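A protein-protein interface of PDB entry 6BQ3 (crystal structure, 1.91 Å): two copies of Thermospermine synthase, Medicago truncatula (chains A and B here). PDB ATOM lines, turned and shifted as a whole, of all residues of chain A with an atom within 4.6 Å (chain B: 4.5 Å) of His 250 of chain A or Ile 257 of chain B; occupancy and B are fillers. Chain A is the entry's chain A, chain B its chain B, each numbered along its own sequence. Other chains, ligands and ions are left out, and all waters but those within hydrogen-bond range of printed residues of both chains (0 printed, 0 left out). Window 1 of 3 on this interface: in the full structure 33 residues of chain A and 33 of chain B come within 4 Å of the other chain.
His 250 of chain A touches Asp 256 of chain B, and with the chains exchanged Asp 256 of chain A touches His 250 of chain B.
His 250 of chain A touches Ile 257 of chain B, and with the chains exchanged Ile 257 of chain A touches His 250 of chain B.
Ile 257 of chain B touches its own counterpart, Ile 257 of chain A.
4 positions are printed for both chains.
Of the 5 pairs that touch across the chains among the printed residues, 5 have their exchanged pair printed and touching as well.
Of the 7 printed residues of chain A, 3 touch a printed residue of chain B.
Among the printed residues, no Asp or Glu carboxylate lies within 4 Å of a Lys or Arg side-chain nitrogen of the other chain.
Among the printed residues, pairs that only touch across the chains: His 250 of chain A with Asp 256 of chain B, His 250 of chain A with Ile 257 of chain B, Asp 256 of chain A with His 250 of chain B, Ile 257 of chain A with His 250 of chain B and Ile 257 of chain A with Ile 257 of chain B.
Of chain B, only Asp 256 and Ile 257 come within 4 Å of His 250 of chain A.
Ile 257 of chain B touches just these residues of chain A: His 250 and Ile 257.
Printed residues of chain A within 4 Å of His 250 of chain B: Asp 256 (3.7 Å) and Ile 257 (3.7 Å).
Printed residues of chain B within 4 Å of Asp 256 of chain A: His 250 (3.7 Å).
Of the printed residues of chain B, Ile 257 of chain A touches His 250 and Ile 257.
Of the printed residues of chain A, Asp 256 of chain B touches His 250.
Ala 221 of chain B touches none of the printed residues of chain A.
Ile 251 of chain A touches none of the printed residues of chain B.
The nearest residue of chain B that does not touch His 250 of chain A is His 250 of chain B (4.03 Å).
The nearest printed residue of chain B that does not touch Ile 257 of chain A is Ala 249 of chain B (6.6 Å).
The backbone NH (N) of Ile 251 of chain A sits at hydrogen-bond distance from the backbone carbonyl oxygen (O) of Asp 256 of chain A (3.1 Å).
N of Ala 221 of chain B is in hydrogen-bond range of O of Ile 257 of chain B.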
ATOM      1  N   ILE A  86      -0.378 -28.261 -18.412  1.00  0.00           N
ATOM      2  CA  ILE A  86      -0.786 -27.488 -19.574  1.00  0.00           C
ATOM      3  C   ILE A  86       0.343 -27.521 -20.604  1.00  0.00           C
ATOM      4  O   ILE A  86       0.123 -27.774 -21.793  1.00  0.00           O
ATOM      5  CB  ILE A  86      -1.055 -26.003 -19.187  1.00  0.00           C
ATOM      6  CG1 ILE A  86      -2.116 -25.930 -18.046  1.00  0.00           C
ATOM      7  CG2 ILE A  86      -1.435 -25.207 -20.445  1.00  0.00           C
ATOM      8  CD1 ILE A  86      -2.267 -24.516 -17.484  1.00  0.00           C
ATOM      9  N   ALA A 249      -0.486 -21.149 -25.565  1.00  0.00           N
ATOM     10  CA  ALA A 249      -1.397 -21.179 -24.408  1.00  0.00           C
ATOM     11  C   ALA A 249      -0.694 -20.586 -23.215  1.00  0.00           C
ATOM     12  O   ALA A 249       0.549 -20.648 -23.119  1.00  0.00           O
ATOM     13  CB  ALA A 249      -1.838 -22.604 -24.123  1.00  0.00           C
ATOM     14  N   HIS A 250      -1.481 -19.927 -22.356  1.00  0.00           N
ATOM     15  CA  HIS A 250      -0.987 -19.336 -21.117  1.00  0.00           C
ATOM     16  C   HIS A 250      -0.415 -20.401 -20.148  1.00  0.00           C
ATOM     17  O   HIS A 250      -1.061 -21.394 -19.865  1.00  0.00           O
ATOM     18  CB  HIS A 250      -2.109 -18.569 -20.410  1.00  0.00           C
ATOM     19  CG  HIS A 250      -1.645 -17.745 -19.245  1.00  0.00           C
ATOM     20  ND1 HIS A 250      -2.171 -17.886 -17.986  1.00  0.00           N
ATOM     21  CD2 HIS A 250      -0.686 -16.792 -19.146  1.00  0.00           C
ATOM     22  CE1 HIS A 250      -1.564 -17.042 -17.164  1.00  0.00           C
ATOM     23  NE2 HIS A 250      -0.661 -16.370 -17.840  1.00  0.00           N
ATOM     24  N   ILE A 251       0.799 -20.175 -19.644  1.00  0.00           N
ATOM     25  CA  ILE A 251       1.307 -20.952 -18.544  1.00  0.00           C
ATOM     26  C   ILE A 251       1.610 -19.982 -17.379  1.00  0.00           C
ATOM     27  O   ILE A 251       2.620 -19.269 -17.424  1.00  0.00           O
ATOM     28  CB  ILE A 251       2.476 -21.830 -18.973  1.00  0.00           C
ATOM     29  CG1 ILE A 251       2.016 -22.817 -20.098  1.00  0.00           C
ATOM     30  CG2 ILE A 251       2.943 -22.648 -17.779  1.00  0.00           C
ATOM     31  CD1 ILE A 251       3.165 -23.356 -20.858  1.00  0.00           C
ATOM     32  N   PRO A 252       0.753 -19.978 -16.338  1.00  0.00           N
ATOM     33  CA  PRO A 252       0.902 -18.995 -15.248  1.00  0.00           C
ATOM     34  C   PRO A 252       2.300 -18.990 -14.648  1.00  0.00           C
ATOM     35  O   PRO A 252       2.875 -17.924 -14.514  1.00  0.00           O
ATOM     36  CB  PRO A 252      -0.160 -19.399 -14.239  1.00  0.00           C
ATOM     37  CG  PRO A 252      -1.208 -20.084 -15.060  1.00  0.00           C
ATOM     38  CD  PRO A 252      -0.467 -20.793 -16.183  1.00  0.00           C
ATOM     39  N   ASP A 256       3.788 -16.031 -18.894  1.00  0.00           N
ATOM     40  CA  ASP A 256       3.523 -15.634 -20.254  1.00  0.00           C
ATOM     41  C   ASP A 256       2.679 -16.642 -20.964  1.00  0.00           C
ATOM     42  O   ASP A 256       2.492 -17.737 -20.484  1.00  0.00           O
ATOM     43  CB  ASP A 256       4.829 -15.449 -21.042  1.00  0.00           C
ATOM     44  CG  ASP A 256       4.759 -14.346 -22.137  1.00  0.00           C
ATOM     45  OD1 ASP A 256       3.642 -13.972 -22.553  1.00  0.00           O
ATOM     46  OD2 ASP A 256       5.853 -13.907 -22.610  1.00  0.00           O
ATOM     47  N   ILE A 257       2.156 -16.226 -22.110  1.00  0.00           N
ATOM     48  CA  ILE A 257       1.716 -17.159 -23.118  1.00  0.00           C
ATOM     49  C   ILE A 257       2.955 -17.877 -23.624  1.00  0.00           C
ATOM     50  O   ILE A 257       4.003 -17.244 -23.868  1.00  0.00           O
ATOM     51  CB  ILE A 257       1.022 -16.449 -24.285  1.00  0.00           C
ATOM     52  CG1 ILE A 257      -0.179 -15.620 -23.834  1.00  0.00           C
ATOM     53  CG2 ILE A 257       0.568 -17.450 -25.325  1.00  0.00           C
ATOM     54  CD1 ILE A 257      -1.142 -16.428 -23.008  1.00  0.00           C
ATOM     55  N   PRO B 220      -9.742 -11.534 -13.522  1.00  0.00           N
ATOM     56  CA  PRO B 220      -8.763 -12.521 -14.040  1.00  0.00           C
ATOM     57  C   PRO B 220      -9.422 -13.749 -14.663  1.00  0.00           C
ATOM     58  O   PRO B 220     -10.424 -14.192 -14.177  1.00  0.00           O
ATOM     59  CB  PRO B 220      -7.978 -12.935 -12.796  1.00  0.00           C
ATOM     60  CG  PRO B 220      -8.165 -11.831 -11.804  1.00  0.00           C
ATOM     61  CD  PRO B 220      -9.525 -11.208 -12.095  1.00  0.00           C
ATOM     62  N   ALA B 221      -8.842 -14.310 -15.720  1.00  0.00           N
ATOM     63  CA  ALA B 221      -9.460 -15.495 -16.363  1.00  0.00           C
ATOM     64  C   ALA B 221      -8.433 -16.571 -16.670  1.00  0.00           C
ATOM     65  O   ALA B 221      -8.560 -17.341 -17.619  1.00  0.00           O
ATOM     66  CB  ALA B 221     -10.201 -15.000 -17.613  1.00  0.00           C
ATOM     67  N   GLY B 222      -7.421 -16.656 -15.822  1.00  0.00           N
ATOM     68  CA  GLY B 222      -6.461 -17.722 -15.889  1.00  0.00           C
ATOM     69  C   GLY B 222      -7.036 -19.064 -15.488  1.00  0.00           C
ATOM     70  O   GLY B 222      -8.116 -19.192 -14.907  1.00  0.00           O
ATOM     71  N   SER B 248     -11.895 -14.139 -23.298  1.00  0.00           N
ATOM     72  CA  SER B 248     -10.677 -13.747 -22.583  1.00  0.00           C
ATOM     73  C   SER B 248      -9.443 -13.580 -23.493  1.00  0.00           C
ATOM     74  O   SER B 248      -9.396 -14.095 -24.595  1.00  0.00           O
ATOM     75  CB  SER B 248     -10.374 -14.790 -21.502  1.00  0.00           C
ATOM     76  OG  SER B 248     -10.094 -16.062 -22.047  1.00  0.00           O
ATOM     77  N   ALA B 249      -8.483 -12.825 -23.003  1.00  0.00           N
ATOM     78  CA  ALA B 249      -7.251 -12.563 -23.713  1.00  0.00           C
ATOM     79  C   ALA B 249      -6.202 -12.204 -22.703  1.00  0.00           C
ATOM     80  O   ALA B 249      -6.511 -11.651 -21.615  1.00  0.00           O
ATOM     81  CB  ALA B 249      -7.425 -11.467 -24.737  1.00  0.00           C
ATOM     82  N   HIS B 250      -4.963 -12.538 -23.053  1.00  0.00           N
ATOM     83  CA  HIS B 250      -3.837 -12.172 -22.272  1.00  0.00           C
ATOM     84  C   HIS B 250      -3.599 -10.654 -22.313  1.00  0.00           C
ATOM     85  O   HIS B 250      -3.604 -10.036 -23.372  1.00  0.00           O
ATOM     86  CB  HIS B 250      -2.619 -12.888 -22.781  1.00  0.00           C
ATOM     87  CG  HIS B 250      -1.434 -12.753 -21.912  1.00  0.00           C
ATOM     88  ND1 HIS B 250      -0.243 -12.218 -22.367  1.00  0.00           N
ATOM     89  CD2 HIS B 250      -1.240 -13.072 -20.607  1.00  0.00           C
ATOM     90  CE1 HIS B 250       0.622 -12.199 -21.369  1.00  0.00           C
ATOM     91  NE2 HIS B 250       0.039 -12.702 -20.292  1.00  0.00           N
ATOM     92  N   ASP B 256      -1.806 -11.646 -16.489  1.00  0.00           N
ATOM     93  CA  ASP B 256      -2.724 -12.775 -16.488  1.00  0.00           C
ATOM     94  C   ASP B 256      -3.557 -12.695 -17.719  1.00  0.00           C
ATOM     95  O   ASP B 256      -3.582 -11.645 -18.381  1.00  0.00           O
ATOM     96  CB  ASP B 256      -3.645 -12.703 -15.242  1.00  0.00           C
ATOM     97  CG  ASP B 256      -4.191 -14.070 -14.814  1.00  0.00           C
ATOM     98  OD1 ASP B 256      -4.018 -15.064 -15.574  1.00  0.00           O
ATOM     99  OD2 ASP B 256      -4.824 -14.140 -13.733  1.00  0.00           O
ATOM    100  N   ILE B 257      -4.319 -13.757 -17.938  1.00  0.00           N
ATOM    101  CA  ILE B 257      -5.436 -13.757 -18.881  1.00  0.00           C
ATOM    102  C   ILE B 257      -6.523 -12.929 -18.209  1.00  0.00           C
ATOM    103  O   ILE B 257      -6.711 -13.063 -16.998  1.00  0.00           O
ATOM    104  CB  ILE B 257      -5.949 -15.186 -19.157  1.00  0.00           C
ATOM    105  CG1 ILE B 257      -4.864 -16.058 -19.808  1.00  0.00           C
ATOM    106  CG2 ILE B 257      -7.212 -15.192 -20.007  1.00  0.00           C
ATOM    107  CD1 ILE B 257      -4.282 -15.540 -21.082  1.00  0.00           C
ATOM    108  N   TRP B 258      -7.203 -12.059 -18.965  1.00  0.00           N
ATOM    109  CA  TRP B 258      -8.294 -11.255 -18.400  1.00  0.00           C
ATOM    110  C   TRP B 258      -9.577 -11.663 -19.087  1.00  0.00           C
ATOM    111  O   TRP B 258      -9.529 -12.158 -20.214  1.00  0.00           O
ATOM    112  CB  TRP B 258      -8.023  -9.751 -18.598  1.00  0.00           C
ATOM    113  CG  TRP B 258      -8.612  -8.944 -17.497  1.00  0.00           C
ATOM    114  CD1 TRP B 258      -9.776  -8.247 -17.511  1.00  0.00           C
ATOM    115  CD2 TRP B 258      -8.134  -8.918 -16.189  1.00  0.00           C
ATOM    116  NE1 TRP B 258     -10.014  -7.737 -16.283  1.00  0.00           N
ATOM    117  CE2 TRP B 258      -8.998  -8.123 -15.449  1.00  0.00           C
ATOM    118  CE3 TRP B 258      -6.980  -9.425 -15.578  1.00  0.00           C
ATOM    119  CZ2 TRP B 258      -8.769  -7.822 -14.098  1.00  0.00           C
ATOM    120  CZ3 TRP B 258      -6.759  -9.124 -14.213  1.00  0.00           C
ATOM    121  CH2 TRP B 258      -7.650  -8.319 -13.510  1.00  0.00           C
ATOM    122  N   GLY B 259     -10.708 -11.431 -18.462  1.00  0.00           N
ATOM    123  CA  GLY B 259     -11.977 -11.866 -18.984  1.00  0.00           C
ATOM    124  C   GLY B 259     -12.994 -10.714 -19.161  1.00  0.00           C
ATOM    125  O   GLY B 259     -12.884  -9.678 -18.484  1.00  0.00           O
